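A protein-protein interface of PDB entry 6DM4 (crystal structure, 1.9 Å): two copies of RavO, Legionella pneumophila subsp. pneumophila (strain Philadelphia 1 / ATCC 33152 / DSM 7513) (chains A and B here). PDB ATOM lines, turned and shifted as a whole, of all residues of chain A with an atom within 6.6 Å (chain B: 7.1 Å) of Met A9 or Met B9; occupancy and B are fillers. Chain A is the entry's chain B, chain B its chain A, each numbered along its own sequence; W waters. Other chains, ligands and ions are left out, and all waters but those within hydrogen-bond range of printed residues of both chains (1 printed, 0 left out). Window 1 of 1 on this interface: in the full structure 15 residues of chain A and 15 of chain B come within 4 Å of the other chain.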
ATOM      1  N   LYS A   4     -16.611 -10.329  20.051  1.00  0.00           N
ATOM      2  CA  LYS A   4     -16.814  -9.195  19.148  1.00  0.00           C
ATOM      3  C   LYS A   4     -15.670  -8.801  18.217  1.00  0.00           C
ATOM      4  O   LYS A   4     -15.904  -8.173  17.185  1.00  0.00           O
ATOM      5  CB  LYS A   4     -17.263  -7.967  19.947  1.00  0.00           C
ATOM      6  CG  LYS A   4     -18.671  -8.073  20.511  1.00  0.00           C
ATOM      7  CD  LYS A   4     -18.939  -6.985  21.537  1.00  0.00           C
ATOM      8  CE  LYS A   4     -20.134  -7.331  22.411  1.00  0.00           C
ATOM      9  NZ  LYS A   4     -21.423  -7.040  21.726  1.00  0.00           N
ATOM     10  N   ILE A   5     -14.441  -9.157  18.567  1.00  0.00           N
ATOM     11  CA  ILE A   5     -13.308  -8.773  17.729  1.00  0.00           C
ATOM     12  C   ILE A   5     -13.401  -9.427  16.360  1.00  0.00           C
ATOM     13  O   ILE A   5     -12.953  -8.856  15.361  1.00  0.00           O
ATOM     14  CB  ILE A   5     -11.969  -9.110  18.417  1.00  0.00           C
ATOM     15  CG1 ILE A   5     -10.809  -8.482  17.635  1.00  0.00           C
ATOM     16  CG2 ILE A   5     -11.782 -10.617  18.555  1.00  0.00           C
ATOM     17  CD1 ILE A   5      -9.438  -8.983  18.042  1.00  0.00           C
ATOM     18  N   TYR A   6     -13.999 -10.617  16.281  1.00  0.00           N
ATOM     19  CA  TYR A   6     -14.039 -11.336  15.012  1.00  0.00           C
ATOM     20  C   TYR A   6     -14.912 -10.619  13.989  1.00  0.00           C
ATOM     21  O   TYR A   6     -14.575 -10.577  12.799  1.00  0.00           O
ATOM     22  CB  TYR A   6     -14.525 -12.763  15.246  1.00  0.00           C
ATOM     23  CG  TYR A   6     -13.569 -13.566  16.089  1.00  0.00           C
ATOM     24  CD1 TYR A   6     -12.223 -13.634  15.758  1.00  0.00           C
ATOM     25  CD2 TYR A   6     -14.002 -14.242  17.222  1.00  0.00           C
ATOM     26  CE1 TYR A   6     -11.332 -14.365  16.526  1.00  0.00           C
ATOM     27  CE2 TYR A   6     -13.116 -14.978  17.995  1.00  0.00           C
ATOM     28  CZ  TYR A   6     -11.783 -15.033  17.643  1.00  0.00           C
ATOM     29  OH  TYR A   6     -10.896 -15.759  18.406  1.00  0.00           O
ATOM     30  N   LYS A   7     -16.003 -10.032  14.472  1.00  0.00           N
ATOM     31  CA  LYS A   7     -16.918  -9.281  13.628  1.00  0.00           C
ATOM     32  C   LYS A   7     -16.222  -8.006  13.170  1.00  0.00           C
ATOM     33  O   LYS A   7     -16.193  -7.703  11.976  1.00  0.00           O
ATOM     34  CB  LYS A   7     -18.200  -8.941  14.390  1.00  0.00           C
ATOM     35  CG  LYS A   7     -19.416  -8.744  13.499  1.00  0.00           C
ATOM     36  CD  LYS A   7     -19.157  -9.254  12.091  1.00  0.00           C
ATOM     37  CE  LYS A   7     -20.342  -8.983  11.179  1.00  0.00           C
ATOM     38  NZ  LYS A   7     -20.573  -7.525  10.984  1.00  0.00           N
ATOM     39  N   VAL A   8     -15.660  -7.258  14.118  1.00  0.00           N
ATOM     40  CA  VAL A   8     -14.948  -6.029  13.767  1.00  0.00           C
ATOM     41  C   VAL A   8     -13.919  -6.312  12.680  1.00  0.00           C
ATOM     42  O   VAL A   8     -13.771  -5.541  11.724  1.00  0.00           O
ATOM     43  CB  VAL A   8     -14.292  -5.406  15.015  1.00  0.00           C
ATOM     44  CG1 VAL A   8     -13.322  -4.304  14.604  1.00  0.00           C
ATOM     45  CG2 VAL A   8     -15.346  -4.862  15.960  1.00  0.00           C
ATOM     46  N   MET A   9     -13.211  -7.440  12.796  1.00  0.00           N
ATOM     47  CA  MET A   9     -12.219  -7.801  11.788  1.00  0.00           C
ATOM     48  C   MET A   9     -12.873  -8.093  10.446  1.00  0.00           C
ATOM     49  O   MET A   9     -12.299  -7.795   9.392  1.00  0.00           O
ATOM     50  CB  MET A   9     -11.400  -9.000  12.267  1.00  0.00           C
ATOM     51  CG  MET A   9     -10.471  -8.694  13.441  1.00  0.00           C
ATOM     52  SD  MET A   9      -9.379  -7.282  13.158  1.00  0.00           S
ATOM     53  CE  MET A   9     -10.260  -6.007  14.017  1.00  0.00           C
ATOM     54  N   GLU A  10     -14.080  -8.662  10.458  1.00  0.00           N
ATOM     55  CA  GLU A  10     -14.790  -8.870   9.203  1.00  0.00           C
ATOM     56  C   GLU A  10     -15.119  -7.542   8.533  1.00  0.00           C
ATOM     57  O   GLU A  10     -14.966  -7.402   7.314  1.00  0.00           O
ATOM     58  CB  GLU A  10     -16.067  -9.671   9.443  1.00  0.00           C
ATOM     59  CG  GLU A  10     -16.688 -10.247   8.181  1.00  0.00           C
ATOM     60  CD  GLU A  10     -18.175  -9.993   8.115  1.00  0.00           C
ATOM     61  OE1 GLU A  10     -18.943 -10.878   7.693  1.00  0.00           O
ATOM     62  OE2 GLU A  10     -18.569  -8.873   8.472  1.00  0.00           O
ATOM     63  N   GLU A  11     -15.576  -6.554   9.311  1.00  0.00           N
ATOM     64  CA  GLU A  11     -15.879  -5.243   8.737  1.00  0.00           C
ATOM     65  C   GLU A  11     -14.660  -4.636   8.072  1.00  0.00           C
ATOM     66  O   GLU A  11     -14.781  -3.977   7.036  1.00  0.00           O
ATOM     67  CB  GLU A  11     -16.411  -4.279   9.801  1.00  0.00           C
ATOM     68  CG  GLU A  11     -17.852  -4.543  10.212  1.00  0.00           C
ATOM     69  CD  GLU A  11     -18.358  -3.601  11.295  1.00  0.00           C
ATOM     70  OE1 GLU A  11     -18.191  -2.371  11.164  1.00  0.00           O
ATOM     71  OE2 GLU A  11     -18.893  -4.126  12.306  1.00  0.00           O
ATOM     72  N   ILE A  12     -13.481  -4.821   8.668  1.00  0.00           N
ATOM     73  CA  ILE A  12     -12.261  -4.215   8.140  1.00  0.00           C
ATOM     74  C   ILE A  12     -11.770  -4.973   6.913  1.00  0.00           C
ATOM     75  O   ILE A  12     -11.493  -4.372   5.867  1.00  0.00           O
ATOM     76  CB  ILE A  12     -11.188  -4.151   9.243  1.00  0.00           C
ATOM     77  CG1 ILE A  12     -11.621  -3.170  10.340  1.00  0.00           C
ATOM     78  CG2 ILE A  12      -9.800  -3.792   8.660  1.00  0.00           C
ATOM     79  CD1 ILE A  12     -10.754  -3.223  11.579  1.00  0.00           C
ATOM     80  N   PHE A  13     -11.678  -6.303   7.015  1.00  0.00           N
ATOM     81  CA  PHE A  13     -11.098  -7.100   5.937  1.00  0.00           C
ATOM     82  C   PHE A  13     -11.917  -7.040   4.649  1.00  0.00           C
ATOM     83  O   PHE A  13     -11.353  -7.130   3.552  1.00  0.00           O
ATOM     84  CB  PHE A  13     -10.947  -8.547   6.392  1.00  0.00           C
ATOM     85  CG  PHE A  13      -9.835  -8.752   7.376  1.00  0.00           C
ATOM     86  CD1 PHE A  13      -8.781  -7.858   7.441  1.00  0.00           C
ATOM     87  CD2 PHE A  13      -9.842  -9.838   8.233  1.00  0.00           C
ATOM     88  CE1 PHE A  13      -7.747  -8.044   8.349  1.00  0.00           C
ATOM     89  CE2 PHE A  13      -8.803 -10.035   9.142  1.00  0.00           C
ATOM     90  CZ  PHE A  13      -7.759  -9.133   9.198  1.00  0.00           C
ATOM     91  N   VAL A  14     -13.247  -6.941   4.753  1.00  0.00           N
ATOM     92  CA  VAL A  14     -14.069  -6.929   3.542  1.00  0.00           C
ATOM     93  C   VAL A  14     -14.042  -5.575   2.852  1.00  0.00           C
ATOM     94  O   VAL A  14     -14.418  -5.479   1.676  1.00  0.00           O
ATOM     95  CB  VAL A  14     -15.540  -7.298   3.816  1.00  0.00           C
ATOM     96  CG1 VAL A  14     -15.664  -8.662   4.488  1.00  0.00           C
ATOM     97  CG2 VAL A  14     -16.213  -6.215   4.643  1.00  0.00           C
ATOM     98  N   TRP A  43      -2.214  -4.882   6.913  1.00  0.00           N
ATOM     99  CA  TRP A  43      -1.799  -5.652   8.078  1.00  0.00           C
ATOM    100  C   TRP A  43      -0.561  -5.007   8.687  1.00  0.00           C
ATOM    101  O   TRP A  43       0.468  -4.880   8.019  1.00  0.00           O
ATOM    102  CB  TRP A  43      -1.517  -7.098   7.662  1.00  0.00           C
ATOM    103  CG  TRP A  43      -1.226  -8.044   8.804  1.00  0.00           C
ATOM    104  CD1 TRP A  43      -0.023  -8.615   9.104  1.00  0.00           C
ATOM    105  CD2 TRP A  43      -2.158  -8.533   9.779  1.00  0.00           C
ATOM    106  NE1 TRP A  43      -0.147  -9.426  10.208  1.00  0.00           N
ATOM    107  CE2 TRP A  43      -1.446  -9.393  10.643  1.00  0.00           C
ATOM    108  CE3 TRP A  43      -3.523  -8.327  10.008  1.00  0.00           C
ATOM    109  CZ2 TRP A  43      -2.054 -10.045  11.717  1.00  0.00           C
ATOM    110  CZ3 TRP A  43      -4.125  -8.975  11.083  1.00  0.00           C
ATOM    111  CH2 TRP A  43      -3.389  -9.822  11.920  1.00  0.00           C
ATOM    112  N   VAL A  56      -4.967  -6.738  17.865  1.00  0.00           N
ATOM    113  CA  VAL A  56      -4.685  -6.938  16.448  1.00  0.00           C
ATOM    114  C   VAL A  56      -4.424  -5.569  15.841  1.00  0.00           C
ATOM    115  O   VAL A  56      -5.233  -4.645  16.001  1.00  0.00           O
ATOM    116  CB  VAL A  56      -5.851  -7.652  15.742  1.00  0.00           C
ATOM    117  CG1 VAL A  56      -5.624  -7.707  14.235  1.00  0.00           C
ATOM    118  CG2 VAL A  56      -6.011  -9.053  16.292  1.00  0.00           C
ATOM    119  N   ILE A  58      -3.829  -2.884  12.818  1.00  0.00           N
ATOM    120  CA  ILE A  58      -4.157  -2.547  11.440  1.00  0.00           C
ATOM    121  C   ILE A  58      -3.619  -1.151  11.180  1.00  0.00           C
ATOM    122  O   ILE A  58      -3.823  -0.245  11.993  1.00  0.00           O
ATOM    123  CB  ILE A  58      -5.677  -2.595  11.182  1.00  0.00           C
ATOM    124  CG1 ILE A  58      -6.228  -3.986  11.502  1.00  0.00           C
ATOM    125  CG2 ILE A  58      -5.999  -2.175   9.745  1.00  0.00           C
ATOM    126  CD1 ILE A  58      -5.660  -5.089  10.626  1.00  0.00           C
ATOM    127  N   GLY A  74      -5.289  -0.404  16.700  1.00  0.00           N
ATOM    128  CA  GLY A  74      -5.351  -1.682  17.376  1.00  0.00           C
ATOM    129  C   GLY A  74      -6.769  -1.977  17.812  1.00  0.00           C
ATOM    130  O   GLY A  74      -7.529  -1.081  18.182  1.00  0.00           O
ATOM    131  N   ILE A  75      -7.118  -3.256  17.760  1.00  0.00           N
ATOM    132  CA  ILE A  75      -8.445  -3.731  18.130  1.00  0.00           C
ATOM    133  C   ILE A  75      -8.268  -4.803  19.191  1.00  0.00           C
ATOM    134  O   ILE A  75      -7.570  -5.799  18.958  1.00  0.00           O
ATOM    135  CB  ILE A  75      -9.216  -4.275  16.919  1.00  0.00           C
ATOM    136  CG1 ILE A  75      -9.365  -3.190  15.847  1.00  0.00           C
ATOM    137  CG2 ILE A  75     -10.586  -4.792  17.351  1.00  0.00           C
ATOM    138  CD1 ILE A  75      -8.285  -3.199  14.784  1.00  0.00           C
ATOM    139  N   ASN A  76      -8.881  -4.598  20.355  1.00  0.00           N
ATOM    140  CA  ASN A  76      -8.757  -5.543  21.452  1.00  0.00           C
ATOM    141  C   ASN A  76      -9.796  -6.657  21.303  1.00  0.00           C
ATOM    142  O   ASN A  76     -10.618  -6.656  20.385  1.00  0.00           O
ATOM    143  CB  ASN A  76      -8.876  -4.825  22.798  1.00  0.00           C
ATOM    144  CG  ASN A  76     -10.246  -4.193  23.024  1.00  0.00           C
ATOM    145  OD1 ASN A  76     -11.164  -4.353  22.223  1.00  0.00           O
ATOM    146  ND2 ASN A  76     -10.381  -3.468  24.129  1.00  0.00           N
ATOM    147  N   GLY A  79     -13.405  -6.057  20.668  1.00  0.00           N
ATOM    148  CA  GLY A  79     -13.726  -5.342  19.452  1.00  0.00           C
ATOM    149  C   GLY A  79     -13.628  -3.837  19.555  1.00  0.00           C
ATOM    150  O   GLY A  79     -14.130  -3.135  18.672  1.00  0.00           O
ATOM    151  N   LYS B   4      -2.943 -16.861  14.114  1.00  0.00           N
ATOM    152  CA  LYS B   4      -3.165 -17.449  12.800  1.00  0.00           C
ATOM    153  C   LYS B   4      -4.638 -17.436  12.411  1.00  0.00           C
ATOM    154  O   LYS B   4      -4.956 -17.492  11.219  1.00  0.00           O
ATOM    155  CB  LYS B   4      -2.598 -18.868  12.761  1.00  0.00           C
ATOM    156  CG  LYS B   4      -1.111 -18.912  13.071  1.00  0.00           C
ATOM    157  CD  LYS B   4      -0.383 -18.023  12.081  1.00  0.00           C
ATOM    158  CE  LYS B   4       0.982 -17.608  12.590  1.00  0.00           C
ATOM    159  NZ  LYS B   4       1.144 -17.788  14.051  1.00  0.00           N
ATOM    160  N   ILE B   5      -5.547 -17.337  13.385  1.00  0.00           N
ATOM    161  CA  ILE B   5      -6.968 -17.248  13.050  1.00  0.00           C
ATOM    162  C   ILE B   5      -7.251 -15.984  12.250  1.00  0.00           C
ATOM    163  O   ILE B   5      -8.050 -15.996  11.306  1.00  0.00           O
ATOM    164  CB  ILE B   5      -7.834 -17.321  14.321  1.00  0.00           C
ATOM    165  CG1 ILE B   5      -9.318 -17.190  13.957  1.00  0.00           C
ATOM    166  CG2 ILE B   5      -7.420 -16.250  15.324  1.00  0.00           C
ATOM    167  CD1 ILE B   5     -10.247 -17.412  15.120  1.00  0.00           C
ATOM    168  N   TYR B   6      -6.605 -14.873  12.606  1.00  0.00           N
ATOM    169  CA  TYR B   6      -6.855 -13.633  11.881  1.00  0.00           C
ATOM    170  C   TYR B   6      -6.310 -13.695  10.461  1.00  0.00           C
ATOM    171  O   TYR B   6      -6.878 -13.080   9.555  1.00  0.00           O
ATOM    172  CB  TYR B   6      -6.259 -12.451  12.642  1.00  0.00           C
ATOM    173  CG  TYR B   6      -6.781 -12.340  14.053  1.00  0.00           C
ATOM    174  CD1 TYR B   6      -8.111 -12.019  14.299  1.00  0.00           C
ATOM    175  CD2 TYR B   6      -5.950 -12.566  15.140  1.00  0.00           C
ATOM    176  CE1 TYR B   6      -8.593 -11.920  15.590  1.00  0.00           C
ATOM    177  CE2 TYR B   6      -6.423 -12.471  16.433  1.00  0.00           C
ATOM    178  CZ  TYR B   6      -7.745 -12.148  16.652  1.00  0.00           C
ATOM    179  OH  TYR B   6      -8.215 -12.051  17.941  1.00  0.00           O
ATOM    180  N   LYS B   7      -5.223 -14.437  10.241  1.00  0.00           N
ATOM    181  CA  LYS B   7      -4.722 -14.583   8.880  1.00  0.00           C
ATOM    182  C   LYS B   7      -5.656 -15.446   8.038  1.00  0.00           C
ATOM    183  O   LYS B   7      -5.840 -15.184   6.843  1.00  0.00           O
ATOM    184  CB  LYS B   7      -3.308 -15.162   8.891  1.00  0.00           C
ATOM    185  CG  LYS B   7      -2.296 -14.314   9.650  1.00  0.00           C
ATOM    186  CD  LYS B   7      -2.415 -12.840   9.291  1.00  0.00           C
ATOM    187  CE  LYS B   7      -1.976 -12.556   7.861  1.00  0.00           C
ATOM    188  NZ  LYS B   7      -2.384 -11.186   7.448  1.00  0.00           N
ATOM    189  N   VAL B   8      -6.261 -16.476   8.640  1.00  0.00           N
ATOM    190  CA  VAL B   8      -7.232 -17.288   7.911  1.00  0.00           C
ATOM    191  C   VAL B   8      -8.490 -16.478   7.623  1.00  0.00           C
ATOM    192  O   VAL B   8      -9.058 -16.557   6.527  1.00  0.00           O
ATOM    193  CB  VAL B   8      -7.553 -18.576   8.691  1.00  0.00           C
ATOM    194  CG1 VAL B   8      -8.573 -19.420   7.936  1.00  0.00           C
ATOM    195  CG2 VAL B   8      -6.282 -19.380   8.941  1.00  0.00           C
ATOM    196  N   MET B   9      -8.941 -15.684   8.598  1.00  0.00           N
ATOM    197  CA  MET B   9     -10.100 -14.825   8.381  1.00  0.00           C
ATOM    198  C   MET B   9      -9.817 -13.792   7.303  1.00  0.00           C
ATOM    199  O   MET B   9     -10.685 -13.501   6.471  1.00  0.00           O
ATOM    200  CB  MET B   9     -10.494 -14.132   9.682  1.00  0.00           C
ATOM    201  CG  MET B   9     -11.149 -15.047  10.692  1.00  0.00           C
ATOM    202  SD  MET B   9     -11.249 -14.254  12.302  1.00  0.00           S
ATOM    203  CE  MET B   9     -11.814 -12.621  11.842  1.00  0.00           C
ATOM    204  N   GLU B  10      -8.612 -13.219   7.310  1.00  0.00           N
ATOM    205  CA  GLU B  10      -8.215 -12.291   6.255  1.00  0.00           C
ATOM    206  C   GLU B  10      -8.354 -12.938   4.886  1.00  0.00           C
ATOM    207  O   GLU B  10      -8.925 -12.347   3.962  1.00  0.00           O
ATOM    208  CB  GLU B  10      -6.774 -11.818   6.484  1.00  0.00           C
ATOM    209  CG  GLU B  10      -6.323 -10.671   5.576  1.00  0.00           C
ATOM    210  CD  GLU B  10      -4.801 -10.538   5.502  1.00  0.00           C
ATOM    211  OE1 GLU B  10      -4.122 -11.578   5.390  1.00  0.00           O
ATOM    212  OE2 GLU B  10      -4.280  -9.405   5.561  1.00  0.00           O
ATOM    213  N   GLU B  11      -7.841 -14.162   4.741  1.00  0.00           N
ATOM    214  CA  GLU B  11      -7.882 -14.845   3.454  1.00  0.00           C
ATOM    215  C   GLU B  11      -9.318 -15.039   2.980  1.00  0.00           C
ATOM    216  O   GLU B  11      -9.609 -14.902   1.788  1.00  0.00           O
ATOM    217  CB  GLU B  11      -7.165 -16.193   3.561  1.00  0.00           C
ATOM    218  CG  GLU B  11      -5.817 -16.239   2.855  1.00  0.00           C
ATOM    219  CD  GLU B  11      -5.102 -17.569   3.033  1.00  0.00           C
ATOM    220  OE1 GLU B  11      -4.622 -17.848   4.152  1.00  0.00           O
ATOM    221  OE2 GLU B  11      -5.018 -18.337   2.051  1.00  0.00           O
ATOM    222  N   ILE B  12     -10.230 -15.344   3.903  1.00  0.00           N
ATOM    223  CA  ILE B  12     -11.621 -15.587   3.526  1.00  0.00           C
ATOM    224  C   ILE B  12     -12.339 -14.275   3.240  1.00  0.00           C
ATOM    225  O   ILE B  12     -13.008 -14.128   2.210  1.00  0.00           O
ATOM    226  CB  ILE B  12     -12.340 -16.395   4.626  1.00  0.00           C
ATOM    227  CG1 ILE B  12     -11.724 -17.788   4.761  1.00  0.00           C
ATOM    228  CG2 ILE B  12     -13.850 -16.511   4.341  1.00  0.00           C
ATOM    229  CD1 ILE B  12     -12.373 -18.630   5.839  1.00  0.00           C
ATOM    230  N   PHE B  13     -12.211 -13.301   4.142  1.00  0.00           N
ATOM    231  CA  PHE B  13     -13.055 -12.113   4.075  1.00  0.00           C
ATOM    232  C   PHE B  13     -12.672 -11.173   2.940  1.00  0.00           C
ATOM    233  O   PHE B  13     -13.505 -10.357   2.527  1.00  0.00           O
ATOM    234  CB  PHE B  13     -13.014 -11.363   5.406  1.00  0.00           C
ATOM    235  CG  PHE B  13     -13.679 -12.099   6.536  1.00  0.00           C
ATOM    236  CD1 PHE B  13     -14.657 -13.046   6.284  1.00  0.00           C
ATOM    237  CD2 PHE B  13     -13.327 -11.841   7.852  1.00  0.00           C
ATOM    238  CE1 PHE B  13     -15.270 -13.725   7.326  1.00  0.00           C
ATOM    239  CE2 PHE B  13     -13.936 -12.516   8.900  1.00  0.00           C
ATOM    240  CZ  PHE B  13     -14.907 -13.458   8.638  1.00  0.00           C
ATOM    241  N   VAL B  14     -11.441 -11.248   2.425  1.00  0.00           N
ATOM    242  CA  VAL B  14     -11.082 -10.411   1.281  1.00  0.00           C
ATOM    243  C   VAL B  14     -11.503 -11.026  -0.043  1.00  0.00           C
ATOM    244  O   VAL B  14     -11.447 -10.345  -1.074  1.00  0.00           O
ATOM    245  CB  VAL B  14      -9.569 -10.109   1.201  1.00  0.00           C
ATOM    246  CG1 VAL B  14      -9.039  -9.572   2.524  1.00  0.00           C
ATOM    247  CG2 VAL B  14      -8.798 -11.354   0.787  1.00  0.00           C
ATOM    248  N   ASP B  15     -11.910 -12.290  -0.051  1.00  0.00           N
ATOM    249  CA  ASP B  15     -12.189 -12.977  -1.301  1.00  0.00           C
ATOM    250  C   ASP B  15     -13.539 -12.534  -1.854  1.00  0.00           C
ATOM    251  O   ASP B  15     -14.480 -12.262  -1.102  1.00  0.00           O
ATOM    252  CB  ASP B  15     -12.173 -14.491  -1.098  1.00  0.00           C
ATOM    253  CG  ASP B  15     -12.286 -15.258  -2.400  1.00  0.00           C
ATOM    254  OD1 ASP B  15     -11.237 -15.580  -2.995  1.00  0.00           O
ATOM    255  OD2 ASP B  15     -13.425 -15.523  -2.840  1.00  0.00           O
ATOM    256  N   TRP B  43     -21.282 -15.117   6.579  1.00  0.00           N
ATOM    257  CA  TRP B  43     -21.209 -15.236   8.028  1.00  0.00           C
ATOM    258  C   TRP B  43     -22.274 -16.221   8.513  1.00  0.00           C
ATOM    259  O   TRP B  43     -23.467 -16.017   8.282  1.00  0.00           O
ATOM    260  CB  TRP B  43     -21.386 -13.856   8.653  1.00  0.00           C
ATOM    261  CG  TRP B  43     -21.120 -13.746  10.130  1.00  0.00           C
ATOM    262  CD1 TRP B  43     -22.056 -13.683  11.119  1.00  0.00           C
ATOM    263  CD2 TRP B  43     -19.843 -13.634  10.778  1.00  0.00           C
ATOM    264  NE1 TRP B  43     -21.447 -13.552  12.339  1.00  0.00           N
ATOM    265  CE2 TRP B  43     -20.089 -13.527  12.162  1.00  0.00           C
ATOM    266  CE3 TRP B  43     -18.518 -13.631  10.328  1.00  0.00           C
ATOM    267  CZ2 TRP B  43     -19.061 -13.413  13.097  1.00  0.00           C
ATOM    268  CZ3 TRP B  43     -17.497 -13.517  11.259  1.00  0.00           C
ATOM    269  CH2 TRP B  43     -17.775 -13.411  12.627  1.00  0.00           C
ATOM    270  N   VAL B  56     -14.820 -19.629  14.888  1.00  0.00           N
ATOM    271  CA  VAL B  56     -15.528 -18.661  14.058  1.00  0.00           C
ATOM    272  C   VAL B  56     -16.139 -19.435  12.900  1.00  0.00           C
ATOM    273  O   VAL B  56     -15.443 -20.201  12.223  1.00  0.00           O
ATOM    274  CB  VAL B  56     -14.584 -17.555  13.557  1.00  0.00           C
ATOM    275  CG1 VAL B  56     -15.296 -16.658  12.548  1.00  0.00           C
ATOM    276  CG2 VAL B  56     -14.067 -16.734  14.729  1.00  0.00           C
ATOM    277  N   ILE B  58     -18.123 -20.027   9.330  1.00  0.00           N
ATOM    278  CA  ILE B  58     -18.334 -19.506   7.985  1.00  0.00           C
ATOM    279  C   ILE B  58     -19.127 -20.542   7.208  1.00  0.00           C
ATOM    280  O   ILE B  58     -18.777 -21.726   7.217  1.00  0.00           O
ATOM    281  CB  ILE B  58     -17.004 -19.208   7.266  1.00  0.00           C
ATOM    282  CG1 ILE B  58     -16.112 -18.308   8.123  1.00  0.00           C
ATOM    283  CG2 ILE B  58     -17.277 -18.582   5.902  1.00  0.00           C
ATOM    284  CD1 ILE B  58     -16.696 -16.955   8.382  1.00  0.00           C
ATOM    285  N   ILE B  75     -13.349 -22.204  12.100  1.00  0.00           N
ATOM    286  CA  ILE B  75     -11.935 -21.902  12.297  1.00  0.00           C
ATOM    287  C   ILE B  75     -11.684 -21.789  13.794  1.00  0.00           C
ATOM    288  O   ILE B  75     -12.347 -20.997  14.474  1.00  0.00           O
ATOM    289  CB  ILE B  75     -11.521 -20.598  11.587  1.00  0.00           C
ATOM    290  CG1 ILE B  75     -12.000 -20.585  10.136  1.00  0.00           C
ATOM    291  CG2 ILE B  75     -10.006 -20.398  11.665  1.00  0.00           C
ATOM    292  CD1 ILE B  75     -12.003 -19.190   9.519  1.00  0.00           C
ATOM    293  N   VAL B 101      -6.124 -21.064   1.755  1.00  0.00           N
ATOM    294  CA  VAL B 101      -7.410 -21.386   2.362  1.00  0.00           C
ATOM    295  C   VAL B 101      -8.528 -21.306   1.331  1.00  0.00           C
ATOM    296  O   VAL B 101      -9.373 -22.205   1.243  1.00  0.00           O
ATOM    297  CB  VAL B 101      -7.683 -20.460   3.561  1.00  0.00           C
ATOM    298  CG1 VAL B 101      -9.085 -20.694   4.104  1.00  0.00           C
ATOM    299  CG2 VAL B 101      -6.638 -20.679   4.644  1.00  0.00           C
HETATM  300  O   HOH W   1      -7.854 -14.312  19.194  1.00  0.00           O
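Water W1 lies within hydrogen-bond range of the side-chain hydroxyl (OH) of Tyr B6 (2.6 Å) and the side-chain hydroxyl (OH) of Tyr A6 (3.5 Å).
Hydrophobic or aromatic side chains of chain A within 4 Å of the printed part of chain B: Ile A5, Tyr A6, Met A9, Phe A13, Val A14, Trp A43 and Val A56.
Of the 17 printed residues of chain B, 9 touch a printed residue of chain A.
Hydrophobic or aromatic side chains of chain B within 4 Å of the printed part of chain A: Ile B5, Tyr B6, Met B9, Phe B13, Val B14, Trp B43 and Val B56.
Among the printed residues, 16 pairs touch across the chains.
Ile A5 touches Tyr B6.
Tyr A6 touches Ile B5.
Tyr A6 touches Val B56 (CG to CG2, 3.5 Å).
CE of Met B9 touches CB of Met A9, at 3.7 Å.
Phe A13 touches Tyr B6.
Phe A13 touches Glu B10.
Val B14 touches Phe A13.
Trp A43 touches Tyr B6 (CH2 to CB, 3.96 Å).
CD2 of Trp A43 touches NZ of Lys B7, at 3.5 Å.
Val A56 touches Tyr B6.
Ile A5 touches Tyr B6, and with the chains exchanged Tyr A6 touches Ile B5.
Phe A13 touches Tyr B6, but with the chains exchanged Tyr A6 does not touch Phe B13 (4.4 Å).
Phe B13 touches its own counterpart, Phe A13.
Trp A43 touches Lys B7, but with the chains exchanged Lys A7 does not touch Trp B43 (4.2 Å).
Of the 16 pairs that touch across the chains among the printed residues, 11 have their exchanged pair printed and touching as well.
NZ of Lys A7 lies within salt-bridge range of OE2 of Glu A10, 3.5 Å away.
The side-chain amino group of Lys B7 is in salt-bridge range of the side-chain carboxylate of Glu B10 (2.7 Å).
N of Val B56 sits at hydrogen-bond distance from O of Ile B75, 2.9 Å away.
The backbone carbonyl oxygen (O) of Val A56 is in hydrogen-bond range of the backbone NH (N) of Ile A75 (2.9 Å).
Of the printed residues of chain B, Tyr A6 touches Ile B5, Tyr B6, Met B9 and Val B56.
Met A9 touches just one residue of chain B: Met B9.
Printed residues of chain B within 4 Å of Val A14: Phe B13.
Gly A74 touches none of the printed residues of chain B.
Printed residues of chain A within 4 Å of Tyr B6: Ile A5 (3.3 Å), Tyr A6 (3.8 Å), Phe A13 (3.6 Å), Trp A43 (3.96 Å) and Val A56 (3.4 Å).
Met B9 touches two residues of chain A.
Asp B15 touches none of the printed residues of chain A.
The nearest residue of chain B that does not touch Met A9 is Tyr B6 (4.2 Å).
The nearest residue of chain A that does not touch Met B9 is Phe A13 (4.1 Å).
The nearest printed residue of chain A that does not touch Glu B10 is Trp A43 (4.2 Å).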
